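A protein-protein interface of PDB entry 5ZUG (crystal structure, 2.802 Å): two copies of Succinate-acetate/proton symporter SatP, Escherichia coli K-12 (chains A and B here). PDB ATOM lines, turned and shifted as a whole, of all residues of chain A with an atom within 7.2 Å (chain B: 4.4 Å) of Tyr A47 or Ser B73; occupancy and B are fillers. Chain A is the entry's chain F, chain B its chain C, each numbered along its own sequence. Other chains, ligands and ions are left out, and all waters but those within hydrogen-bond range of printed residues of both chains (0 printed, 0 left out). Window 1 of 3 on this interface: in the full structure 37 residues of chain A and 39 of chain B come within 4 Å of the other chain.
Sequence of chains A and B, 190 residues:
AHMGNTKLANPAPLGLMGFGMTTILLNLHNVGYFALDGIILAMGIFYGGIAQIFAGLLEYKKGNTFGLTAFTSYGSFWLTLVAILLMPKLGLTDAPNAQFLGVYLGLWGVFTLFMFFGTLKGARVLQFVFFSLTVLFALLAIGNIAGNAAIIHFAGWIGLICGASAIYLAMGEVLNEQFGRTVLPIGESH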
ATOM      1  N   PRO A  13       3.696   6.604  -2.150  1.00  0.00           N
ATOM      2  CA  PRO A  13       4.034   7.797  -2.952  1.00  0.00           C
ATOM      3  C   PRO A  13       5.474   7.806  -3.468  1.00  0.00           C
ATOM      4  O   PRO A  13       5.700   8.161  -4.631  1.00  0.00           O
ATOM      5  CB  PRO A  13       3.754   8.951  -1.982  1.00  0.00           C
ATOM      6  CG  PRO A  13       2.695   8.428  -1.103  1.00  0.00           C
ATOM      7  CD  PRO A  13       3.024   6.976  -0.895  1.00  0.00           C
ATOM      8  N   LEU A  14       6.458   7.422  -2.642  1.00  0.00           N
ATOM      9  CA  LEU A  14       7.835   7.332  -3.121  1.00  0.00           C
ATOM     10  C   LEU A  14       7.949   6.349  -4.279  1.00  0.00           C
ATOM     11  O   LEU A  14       8.529   6.668  -5.327  1.00  0.00           O
ATOM     12  CB  LEU A  14       8.763   6.891  -1.997  1.00  0.00           C
ATOM     13  CG  LEU A  14      10.170   6.576  -2.522  1.00  0.00           C
ATOM     14  CD1 LEU A  14      10.904   7.844  -3.014  1.00  0.00           C
ATOM     15  CD2 LEU A  14      11.020   5.717  -1.596  1.00  0.00           C
ATOM     16  N   GLY A  15       7.417   5.136  -4.104  1.00  0.00           N
ATOM     17  CA  GLY A  15       7.504   4.150  -5.171  1.00  0.00           C
ATOM     18  C   GLY A  15       6.751   4.573  -6.417  1.00  0.00           C
ATOM     19  O   GLY A  15       7.255   4.438  -7.535  1.00  0.00           O
ATOM     20  N   LEU A  16       5.555   5.141  -6.239  1.00  0.00           N
ATOM     21  CA  LEU A  16       4.794   5.619  -7.390  1.00  0.00           C
ATOM     22  C   LEU A  16       5.496   6.777  -8.094  1.00  0.00           C
ATOM     23  O   LEU A  16       5.553   6.818  -9.330  1.00  0.00           O
ATOM     24  CB  LEU A  16       3.396   6.050  -6.964  1.00  0.00           C
ATOM     25  CG  LEU A  16       2.372   4.977  -6.638  1.00  0.00           C
ATOM     26  CD1 LEU A  16       1.175   5.647  -5.961  1.00  0.00           C
ATOM     27  CD2 LEU A  16       1.977   4.164  -7.857  1.00  0.00           C
ATOM     28  N   MET A  17       6.030   7.727  -7.326  1.00  0.00           N
ATOM     29  CA  MET A  17       6.788   8.811  -7.928  1.00  0.00           C
ATOM     30  C   MET A  17       7.963   8.262  -8.736  1.00  0.00           C
ATOM     31  O   MET A  17       8.173   8.638  -9.897  1.00  0.00           O
ATOM     32  CB  MET A  17       7.291   9.751  -6.834  1.00  0.00           C
ATOM     33  CG  MET A  17       6.266  10.688  -6.269  1.00  0.00           C
ATOM     34  SD  MET A  17       5.471  11.632  -7.557  1.00  0.00           S
ATOM     35  CE  MET A  17       6.896  12.234  -8.439  1.00  0.00           C
ATOM     36  N   GLY A  18       8.745   7.368  -8.132  1.00  0.00           N
ATOM     37  CA  GLY A  18       9.876   6.804  -8.846  1.00  0.00           C
ATOM     38  C   GLY A  18       9.447   6.131 -10.133  1.00  0.00           C
ATOM     39  O   GLY A  18       9.977   6.420 -11.211  1.00  0.00           O
ATOM     40  N   PHE A  19       8.483   5.211 -10.026  1.00  0.00           N
ATOM     41  CA  PHE A  19       7.930   4.533 -11.197  1.00  0.00           C
ATOM     42  C   PHE A  19       7.389   5.513 -12.236  1.00  0.00           C
ATOM     43  O   PHE A  19       7.662   5.384 -13.437  1.00  0.00           O
ATOM     44  CB  PHE A  19       6.811   3.597 -10.766  1.00  0.00           C
ATOM     45  CG  PHE A  19       5.973   3.128 -11.902  1.00  0.00           C
ATOM     46  CD1 PHE A  19       6.331   1.994 -12.607  1.00  0.00           C
ATOM     47  CD2 PHE A  19       4.832   3.833 -12.283  1.00  0.00           C
ATOM     48  CE1 PHE A  19       5.549   1.545 -13.657  1.00  0.00           C
ATOM     49  CE2 PHE A  19       4.054   3.407 -13.346  1.00  0.00           C
ATOM     50  CZ  PHE A  19       4.409   2.254 -14.032  1.00  0.00           C
ATOM     51  N   GLY A  20       6.526   6.432 -11.797  1.00  0.00           N
ATOM     52  CA  GLY A  20       5.819   7.270 -12.747  1.00  0.00           C
ATOM     53  C   GLY A  20       6.752   8.198 -13.493  1.00  0.00           C
ATOM     54  O   GLY A  20       6.756   8.229 -14.727  1.00  0.00           O
ATOM     55  N   MET A  21       7.581   8.938 -12.752  1.00  0.00           N
ATOM     56  CA  MET A  21       8.489   9.897 -13.371  1.00  0.00           C
ATOM     57  C   MET A  21       9.437   9.203 -14.344  1.00  0.00           C
ATOM     58  O   MET A  21       9.666   9.690 -15.458  1.00  0.00           O
ATOM     59  CB  MET A  21       9.228  10.672 -12.280  1.00  0.00           C
ATOM     60  CG  MET A  21       9.720  12.016 -12.748  1.00  0.00           C
ATOM     61  SD  MET A  21      10.544  13.041 -11.498  1.00  0.00           S
ATOM     62  CE  MET A  21       9.142  13.639 -10.587  1.00  0.00           C
ATOM     63  N   THR A  22       9.956   8.041 -13.962  1.00  0.00           N
ATOM     64  CA  THR A  22      10.861   7.300 -14.839  1.00  0.00           C
ATOM     65  C   THR A  22      10.143   6.842 -16.102  1.00  0.00           C
ATOM     66  O   THR A  22      10.721   6.844 -17.194  1.00  0.00           O
ATOM     67  CB  THR A  22      11.414   6.073 -14.091  1.00  0.00           C
ATOM     68  OG1 THR A  22      12.038   6.483 -12.868  1.00  0.00           O
ATOM     69  CG2 THR A  22      12.420   5.286 -14.935  1.00  0.00           C
ATOM     70  N   LEU A  41      18.222   6.738 -18.417  1.00  0.00           N
ATOM     71  CA  LEU A  41      19.092   5.736 -17.792  1.00  0.00           C
ATOM     72  C   LEU A  41      19.393   6.056 -16.327  1.00  0.00           C
ATOM     73  O   LEU A  41      19.408   5.146 -15.483  1.00  0.00           O
ATOM     74  CB  LEU A  41      20.390   5.587 -18.584  1.00  0.00           C
ATOM     75  CG  LEU A  41      20.258   5.003 -19.991  1.00  0.00           C
ATOM     76  CD1 LEU A  41      21.595   5.029 -20.703  1.00  0.00           C
ATOM     77  CD2 LEU A  41      19.718   3.568 -19.902  1.00  0.00           C
ATOM     78  N   ALA A  42      19.673   7.329 -16.008  1.00  0.00           N
ATOM     79  CA  ALA A  42      19.911   7.708 -14.618  1.00  0.00           C
ATOM     80  C   ALA A  42      18.666   7.481 -13.775  1.00  0.00           C
ATOM     81  O   ALA A  42      18.703   6.765 -12.763  1.00  0.00           O
ATOM     82  CB  ALA A  42      20.335   9.173 -14.533  1.00  0.00           C
ATOM     83  N   MET A  43      17.536   8.039 -14.229  1.00  0.00           N
ATOM     84  CA  MET A  43      16.264   7.869 -13.540  1.00  0.00           C
ATOM     85  C   MET A  43      15.944   6.394 -13.380  1.00  0.00           C
ATOM     86  O   MET A  43      15.489   5.959 -12.317  1.00  0.00           O
ATOM     87  CB  MET A  43      15.163   8.598 -14.314  1.00  0.00           C
ATOM     88  CG  MET A  43      15.224  10.124 -14.227  1.00  0.00           C
ATOM     89  SD  MET A  43      14.743  10.785 -12.617  1.00  0.00           S
ATOM     90  CE  MET A  43      12.982  10.720 -12.797  1.00  0.00           C
ATOM     91  N   GLY A  44      16.191   5.601 -14.414  1.00  0.00           N
ATOM     92  CA  GLY A  44      15.947   4.180 -14.282  1.00  0.00           C
ATOM     93  C   GLY A  44      16.813   3.514 -13.234  1.00  0.00           C
ATOM     94  O   GLY A  44      16.394   2.535 -12.612  1.00  0.00           O
ATOM     95  N   ILE A  45      18.035   4.021 -13.032  1.00  0.00           N
ATOM     96  CA  ILE A  45      18.927   3.460 -12.012  1.00  0.00           C
ATOM     97  C   ILE A  45      18.450   3.839 -10.612  1.00  0.00           C
ATOM     98  O   ILE A  45      18.278   2.979  -9.743  1.00  0.00           O
ATOM     99  CB  ILE A  45      20.390   3.895 -12.241  1.00  0.00           C
ATOM    100  CG1 ILE A  45      20.995   3.194 -13.468  1.00  0.00           C
ATOM    101  CG2 ILE A  45      21.220   3.625 -10.996  1.00  0.00           C
ATOM    102  CD1 ILE A  45      22.354   3.775 -13.943  1.00  0.00           C
ATOM    103  N   PHE A  46      18.259   5.132 -10.361  1.00  0.00           N
ATOM    104  CA  PHE A  46      18.112   5.579  -8.993  1.00  0.00           C
ATOM    105  C   PHE A  46      16.665   5.783  -8.559  1.00  0.00           C
ATOM    106  O   PHE A  46      16.337   5.493  -7.395  1.00  0.00           O
ATOM    107  CB  PHE A  46      18.918   6.866  -8.762  1.00  0.00           C
ATOM    108  CG  PHE A  46      20.423   6.674  -8.907  1.00  0.00           C
ATOM    109  CD1 PHE A  46      21.161   6.039  -7.906  1.00  0.00           C
ATOM    110  CD2 PHE A  46      21.108   7.173 -10.019  1.00  0.00           C
ATOM    111  CE1 PHE A  46      22.531   5.857  -8.041  1.00  0.00           C
ATOM    112  CE2 PHE A  46      22.481   7.005 -10.148  1.00  0.00           C
ATOM    113  CZ  PHE A  46      23.188   6.346  -9.165  1.00  0.00           C
ATOM    114  N   TYR A  47      15.774   6.209  -9.458  1.00  0.00           N
ATOM    115  CA  TYR A  47      14.430   6.593  -9.043  1.00  0.00           C
ATOM    116  C   TYR A  47      13.385   5.536  -9.362  1.00  0.00           C
ATOM    117  O   TYR A  47      12.646   5.115  -8.473  1.00  0.00           O
ATOM    118  CB  TYR A  47      14.053   7.924  -9.690  1.00  0.00           C
ATOM    119  CG  TYR A  47      12.978   8.695  -8.957  1.00  0.00           C
ATOM    120  CD1 TYR A  47      12.916   8.699  -7.571  1.00  0.00           C
ATOM    121  CD2 TYR A  47      12.060   9.460  -9.653  1.00  0.00           C
ATOM    122  CE1 TYR A  47      11.948   9.422  -6.904  1.00  0.00           C
ATOM    123  CE2 TYR A  47      11.095  10.180  -9.002  1.00  0.00           C
ATOM    124  CZ  TYR A  47      11.038  10.163  -7.628  1.00  0.00           C
ATOM    125  OH  TYR A  47      10.057  10.901  -7.000  1.00  0.00           O
ATOM    126  N   GLY A  48      13.297   5.095 -10.610  1.00  0.00           N
ATOM    127  CA  GLY A  48      12.423   3.977 -10.913  1.00  0.00           C
ATOM    128  C   GLY A  48      12.964   2.632 -10.464  1.00  0.00           C
ATOM    129  O   GLY A  48      12.185   1.684 -10.309  1.00  0.00           O
ATOM    130  N   GLY A  49      14.269   2.530 -10.215  1.00  0.00           N
ATOM    131  CA  GLY A  49      14.800   1.246  -9.801  1.00  0.00           C
ATOM    132  C   GLY A  49      15.045   1.168  -8.304  1.00  0.00           C
ATOM    133  O   GLY A  49      14.260   0.524  -7.586  1.00  0.00           O
ATOM    134  N   ILE A  50      16.114   1.822  -7.821  1.00  0.00           N
ATOM    135  CA  ILE A  50      16.491   1.736  -6.406  1.00  0.00           C
ATOM    136  C   ILE A  50      15.364   2.270  -5.522  1.00  0.00           C
ATOM    137  O   ILE A  50      14.900   1.595  -4.589  1.00  0.00           O
ATOM    138  CB  ILE A  50      17.797   2.508  -6.130  1.00  0.00           C
ATOM    139  CG1 ILE A  50      19.001   1.997  -6.948  1.00  0.00           C
ATOM    140  CG2 ILE A  50      18.098   2.456  -4.647  1.00  0.00           C
ATOM    141  CD1 ILE A  50      19.495   0.619  -6.597  1.00  0.00           C
ATOM    142  N   ALA A  51      14.926   3.509  -5.790  1.00  0.00           N
ATOM    143  CA  ALA A  51      13.952   4.154  -4.921  1.00  0.00           C
ATOM    144  C   ALA A  51      12.683   3.334  -4.823  1.00  0.00           C
ATOM    145  O   ALA A  51      12.099   3.209  -3.741  1.00  0.00           O
ATOM    146  CB  ALA A  51      13.644   5.561  -5.423  1.00  0.00           C
ATOM    147  N   GLN A  52      12.268   2.716  -5.927  1.00  0.00           N
ATOM    148  CA  GLN A  52      11.075   1.877  -5.870  1.00  0.00           C
ATOM    149  C   GLN A  52      11.327   0.581  -5.123  1.00  0.00           C
ATOM    150  O   GLN A  52      10.425   0.076  -4.456  1.00  0.00           O
ATOM    151  CB  GLN A  52      10.554   1.568  -7.266  1.00  0.00           C
ATOM    152  CG  GLN A  52       9.121   1.088  -7.267  1.00  0.00           C
ATOM    153  CD  GLN A  52       8.598   0.860  -8.660  1.00  0.00           C
ATOM    154  OE1 GLN A  52       7.508   0.315  -8.838  1.00  0.00           O
ATOM    155  NE2 GLN A  52       9.353   1.311  -9.661  1.00  0.00           N
ATOM    156  N   ILE A  53      12.532   0.030  -5.219  1.00  0.00           N
ATOM    157  CA  ILE A  53      12.841  -1.165  -4.444  1.00  0.00           C
ATOM    158  C   ILE A  53      12.757  -0.868  -2.954  1.00  0.00           C
ATOM    159  O   ILE A  53      12.318  -1.705  -2.157  1.00  0.00           O
ATOM    160  CB  ILE A  53      14.211  -1.721  -4.861  1.00  0.00           C
ATOM    161  CG1 ILE A  53      14.096  -2.345  -6.254  1.00  0.00           C
ATOM    162  CG2 ILE A  53      14.698  -2.768  -3.874  1.00  0.00           C
ATOM    163  CD1 ILE A  53      15.399  -2.644  -6.878  1.00  0.00           C
ATOM    164  N   GLY A  75      10.871  -1.881  -9.666  1.00  0.00           N
ATOM    165  CA  GLY A  75      12.208  -1.326  -9.523  1.00  0.00           C
ATOM    166  C   GLY A  75      13.274  -2.265 -10.042  1.00  0.00           C
ATOM    167  O   GLY A  75      14.239  -1.833 -10.676  1.00  0.00           O
ATOM    168  N   TRP A  78      13.268  -2.102 -13.876  1.00  0.00           N
ATOM    169  CA  TRP A  78      14.013  -0.936 -14.339  1.00  0.00           C
ATOM    170  C   TRP A  78      15.519  -1.148 -14.220  1.00  0.00           C
ATOM    171  O   TRP A  78      16.292  -0.621 -15.034  1.00  0.00           O
ATOM    172  CB  TRP A  78      13.578   0.291 -13.554  1.00  0.00           C
ATOM    173  CG  TRP A  78      12.304   0.864 -14.029  1.00  0.00           C
ATOM    174  CD1 TRP A  78      11.107   0.779 -13.407  1.00  0.00           C
ATOM    175  CD2 TRP A  78      12.087   1.654 -15.215  1.00  0.00           C
ATOM    176  NE1 TRP A  78      10.148   1.451 -14.124  1.00  0.00           N
ATOM    177  CE2 TRP A  78      10.722   1.994 -15.241  1.00  0.00           C
ATOM    178  CE3 TRP A  78      12.911   2.093 -16.260  1.00  0.00           C
ATOM    179  CZ2 TRP A  78      10.155   2.756 -16.269  1.00  0.00           C
ATOM    180  CZ3 TRP A  78      12.344   2.853 -17.282  1.00  0.00           C
ATOM    181  CH2 TRP A  78      10.981   3.179 -17.273  1.00  0.00           C
ATOM    182  N   ILE A 167       2.077   9.308 -10.930  1.00  0.00           N
ATOM    183  CA  ILE A 167       2.424  10.542 -10.239  1.00  0.00           C
ATOM    184  C   ILE A 167       1.191  11.140  -9.587  1.00  0.00           C
ATOM    185  O   ILE A 167       1.231  11.546  -8.417  1.00  0.00           O
ATOM    186  CB  ILE A 167       3.081  11.553 -11.192  1.00  0.00           C
ATOM    187  CG1 ILE A 167       4.452  11.057 -11.658  1.00  0.00           C
ATOM    188  CG2 ILE A 167       3.143  12.918 -10.538  1.00  0.00           C
ATOM    189  CD1 ILE A 167       5.171  12.029 -12.595  1.00  0.00           C
ATOM    190  N   MET A 171       0.764  11.686  -5.546  1.00  0.00           N
ATOM    191  CA  MET A 171       0.482  12.983  -4.957  1.00  0.00           C
ATOM    192  C   MET A 171      -0.897  13.035  -4.305  1.00  0.00           C
ATOM    193  O   MET A 171      -1.102  13.803  -3.358  1.00  0.00           O
ATOM    194  CB  MET A 171       0.680  14.066  -6.005  1.00  0.00           C
ATOM    195  CG  MET A 171       2.168  14.276  -6.342  1.00  0.00           C
ATOM    196  SD  MET A 171       3.240  14.616  -4.896  1.00  0.00           S
ATOM    197  CE  MET A 171       3.865  12.981  -4.455  1.00  0.00           C
ATOM    198  N   THR B  69       8.712  10.586   1.480  1.00  0.00           N
ATOM    199  CA  THR B  69       8.609  10.764   0.040  1.00  0.00           C
ATOM    200  C   THR B  69       9.517  11.879  -0.464  1.00  0.00           C
ATOM    201  O   THR B  69      10.237  11.701  -1.455  1.00  0.00           O
ATOM    202  CB  THR B  69       7.153  11.016  -0.333  1.00  0.00           C
ATOM    203  OG1 THR B  69       6.355   9.915   0.158  1.00  0.00           O
ATOM    204  CG2 THR B  69       7.015  11.140  -1.857  1.00  0.00           C
ATOM    205  N   ALA B  70       9.550  13.012   0.226  1.00  0.00           N
ATOM    206  CA  ALA B  70      10.346  14.124  -0.281  1.00  0.00           C
ATOM    207  C   ALA B  70      11.846  13.828  -0.197  1.00  0.00           C
ATOM    208  O   ALA B  70      12.488  13.674  -1.238  1.00  0.00           O
ATOM    209  CB  ALA B  70       9.976  15.419   0.443  1.00  0.00           C
ATOM    210  N   PHE B  71      12.399  13.699   1.020  1.00  0.00           N
ATOM    211  CA  PHE B  71      13.842  13.476   1.202  1.00  0.00           C
ATOM    212  C   PHE B  71      14.373  12.316   0.356  1.00  0.00           C
ATOM    213  O   PHE B  71      15.479  12.388  -0.195  1.00  0.00           O
ATOM    214  CB  PHE B  71      14.154  13.160   2.664  1.00  0.00           C
ATOM    215  CG  PHE B  71      14.182  14.337   3.563  1.00  0.00           C
ATOM    216  CD1 PHE B  71      14.896  15.466   3.220  1.00  0.00           C
ATOM    217  CD2 PHE B  71      13.595  14.272   4.800  1.00  0.00           C
ATOM    218  CE1 PHE B  71      14.952  16.548   4.067  1.00  0.00           C
ATOM    219  CE2 PHE B  71      13.660  15.347   5.659  1.00  0.00           C
ATOM    220  CZ  PHE B  71      14.340  16.487   5.288  1.00  0.00           C
ATOM    221  N   THR B  72      13.632  11.214   0.297  1.00  0.00           N
ATOM    222  CA  THR B  72      14.090  10.080  -0.487  1.00  0.00           C
ATOM    223  C   THR B  72      14.072  10.394  -1.977  1.00  0.00           C
ATOM    224  O   THR B  72      14.964   9.956  -2.717  1.00  0.00           O
ATOM    225  CB  THR B  72      13.242   8.855  -0.183  1.00  0.00           C
ATOM    226  OG1 THR B  72      13.043   8.770   1.239  1.00  0.00           O
ATOM    227  CG2 THR B  72      13.950   7.606  -0.668  1.00  0.00           C
ATOM    228  N   SER B  73      13.060  11.129  -2.453  1.00  0.00           N
ATOM    229  CA  SER B  73      12.995  11.421  -3.884  1.00  0.00           C
ATOM    230  C   SER B  73      14.087  12.391  -4.311  1.00  0.00           C
ATOM    231  O   SER B  73      14.693  12.215  -5.377  1.00  0.00           O
ATOM    232  CB  SER B  73      11.616  11.945  -4.263  1.00  0.00           C
ATOM    233  OG  SER B  73      10.655  10.914  -4.119  1.00  0.00           O
ATOM    234  N   TYR B  74      14.384  13.402  -3.487  1.00  0.00           N
ATOM    235  CA  TYR B  74      15.380  14.391  -3.904  1.00  0.00           C
ATOM    236  C   TYR B  74      16.806  13.843  -3.810  1.00  0.00           C
ATOM    237  O   TYR B  74      17.642  14.146  -4.668  1.00  0.00           O
ATOM    238  CB  TYR B  74      15.238  15.659  -3.063  1.00  0.00           C
ATOM    239  CG  TYR B  74      13.945  16.375  -3.347  1.00  0.00           C
ATOM    240  CD1 TYR B  74      13.602  16.742  -4.639  1.00  0.00           C
ATOM    241  CD2 TYR B  74      13.018  16.604  -2.330  1.00  0.00           C
ATOM    242  CE1 TYR B  74      12.398  17.378  -4.903  1.00  0.00           C
ATOM    243  CE2 TYR B  74      11.808  17.227  -2.581  1.00  0.00           C
ATOM    244  CZ  TYR B  74      11.499  17.612  -3.874  1.00  0.00           C
ATOM    245  OH  TYR B  74      10.291  18.230  -4.132  1.00  0.00           O
ATOM    246  N   GLY B  75      17.092  13.008  -2.802  1.00  0.00           N
ATOM    247  CA  GLY B  75      18.377  12.330  -2.761  1.00  0.00           C
ATOM    248  C   GLY B  75      18.610  11.488  -3.995  1.00  0.00           C
ATOM    249  O   GLY B  75      19.718  11.466  -4.542  1.00  0.00           O
ATOM    250  N   SER B  76      17.567  10.783  -4.455  1.00  0.00           N
ATOM    251  CA  SER B  76      17.662  10.057  -5.723  1.00  0.00           C
ATOM    252  C   SER B  76      17.808  11.002  -6.908  1.00  0.00           C
ATOM    253  O   SER B  76      18.491  10.676  -7.890  1.00  0.00           O
ATOM    254  CB  SER B  76      16.460   9.147  -5.912  1.00  0.00           C
ATOM    255  OG  SER B  76      16.481   8.133  -4.942  1.00  0.00           O
ATOM    256  N   PHE B  77      17.129  12.154  -6.866  1.00  0.00           N
ATOM    257  CA  PHE B  77      17.291  13.135  -7.935  1.00  0.00           C
ATOM    258  C   PHE B  77      18.752  13.556  -8.077  1.00  0.00           C
ATOM    259  O   PHE B  77      19.312  13.550  -9.188  1.00  0.00           O
ATOM    260  CB  PHE B  77      16.395  14.343  -7.687  1.00  0.00           C
ATOM    261  CG  PHE B  77      16.893  15.608  -8.340  1.00  0.00           C
ATOM    262  CD1 PHE B  77      16.725  15.815  -9.706  1.00  0.00           C
ATOM    263  CD2 PHE B  77      17.469  16.618  -7.578  1.00  0.00           C
ATOM    264  CE1 PHE B  77      17.177  16.981 -10.310  1.00  0.00           C
ATOM    265  CE2 PHE B  77      17.906  17.789  -8.171  1.00  0.00           C
ATOM    266  CZ  PHE B  77      17.756  17.974  -9.539  1.00  0.00           C
ATOM    267  N   TRP B 108      10.655  16.888 -12.309  1.00  0.00           N
ATOM    268  CA  TRP B 108      11.015  17.090 -10.910  1.00  0.00           C
ATOM    269  C   TRP B 108      10.357  18.348 -10.358  1.00  0.00           C
ATOM    270  O   TRP B 108      10.035  18.412  -9.166  1.00  0.00           O
ATOM    271  CB  TRP B 108      12.548  17.129 -10.753  1.00  0.00           C
ATOM    272  CG  TRP B 108      13.155  15.749 -10.845  1.00  0.00           C
ATOM    273  CD1 TRP B 108      13.796  15.191 -11.920  1.00  0.00           C
ATOM    274  CD2 TRP B 108      13.106  14.732  -9.843  1.00  0.00           C
ATOM    275  NE1 TRP B 108      14.166  13.899 -11.633  1.00  0.00           N
ATOM    276  CE2 TRP B 108      13.749  13.594 -10.365  1.00  0.00           C
ATOM    277  CE3 TRP B 108      12.591  14.679  -8.549  1.00  0.00           C
ATOM    278  CZ2 TRP B 108      13.893  12.424  -9.637  1.00  0.00           C
ATOM    279  CZ3 TRP B 108      12.728  13.513  -7.833  1.00  0.00           C
ATOM    280  CH2 TRP B 108      13.377  12.402  -8.378  1.00  0.00           C
ATOM    281  N   PHE B 111       6.661  17.473  -9.201  1.00  0.00           N
ATOM    282  CA  PHE B 111       6.702  16.765  -7.922  1.00  0.00           C
ATOM    283  C   PHE B 111       6.809  17.755  -6.778  1.00  0.00           C
ATOM    284  O   PHE B 111       6.064  17.666  -5.799  1.00  0.00           O
ATOM    285  CB  PHE B 111       7.867  15.771  -7.878  1.00  0.00           C
ATOM    286  CG  PHE B 111       8.120  15.183  -6.500  1.00  0.00           C
ATOM    287  CD1 PHE B 111       7.244  14.250  -5.948  1.00  0.00           C
ATOM    288  CD2 PHE B 111       9.225  15.579  -5.744  1.00  0.00           C
ATOM    289  CE1 PHE B 111       7.474  13.705  -4.684  1.00  0.00           C
ATOM    290  CE2 PHE B 111       9.450  15.051  -4.474  1.00  0.00           C
ATOM    291  CZ  PHE B 111       8.568  14.108  -3.945  1.00  0.00           C
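The side-chain hydroxyl of Tyr A47 sits at hydrogen-bond distance from the side-chain hydroxyl of Ser B73, 2.9 Å away.
NE1 of Trp B108 sits close to SD of Met A21 (3.7 Å).
SD of Met A43 lies within hydrogen-bond range of NE1 of Trp B108 (3.3 Å).
OG of Ser B76 is in hydrogen-bond range of O of Thr B72 (3.3 Å).
N of Ala A51 lies within hydrogen-bond range of O of Phe A46.
OG of Ser B73 sits at hydrogen-bond distance from O of Thr B69 (2.8 Å).
The backbone NH (N) of Gly A48 is in hydrogen-bond range of the backbone carbonyl oxygen (O) of Met A43.
Among the printed residues, pairs that only touch across the chains: Pro A13 with Thr B69 (3.5 Å), Leu A14 with Thr B69 (3.8 Å), Leu A14 with Thr B72 (3.6 Å), Leu A14 with Ser B73 (3.3 Å), Met A17 with Phe B111 (3.2 Å), Met A21 with Phe B111 (3.7 Å), Phe A46 with Ser B76 (3.6 Å), Tyr A47 with Ser B76 (3.9 Å), Tyr A47 with Trp B108 (3.2 Å), Ala A51 with Ser B76 (3.9 Å) and Met A171 with Phe B111 (3.7 Å).
Of the printed residues of chain B, Pro A13 touches Thr B69.
Of chain B, only Ser B73 (2.9 Å), Ser B76 (3.9 Å) and Trp B108 (3.2 Å) come within 4 Å of Tyr A47.
Printed residues of chain B within 4 Å of Ala A51: Ser B76.
Of the printed residues of chain A, Thr B72 touches Leu A14.
Of chain A, only Leu A14 and Tyr A47 come within 4 Å of Ser B73.
The nearest printed residue of chain B that does not touch Tyr A47 is Phe B111 (4.5 Å).
The nearest printed residue of chain B that does not touch Met A17 is Ser B73 (4.5 Å).
Of the 11 printed residues of chain B, 6 touch a printed residue of chain A.
Hydrophobic or aromatic side chains of chain B that line the printed part of chain A: Trp B108 and Phe B111.
Of the 27 printed residues of chain A, 9 touch a printed residue of chain B.
Printed residues of chain A that touch a printed residue of chain B: Pro A13, Leu A14, Met A17, Met A21, Met A43, Phe A46, Tyr A47, Ala A51 and Met A171.
Among the printed residues, no Asp or Glu carboxylate lies within 4 Å of a Lys or Arg side-chain nitrogen of the other chain.
1 position is printed for both chains.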
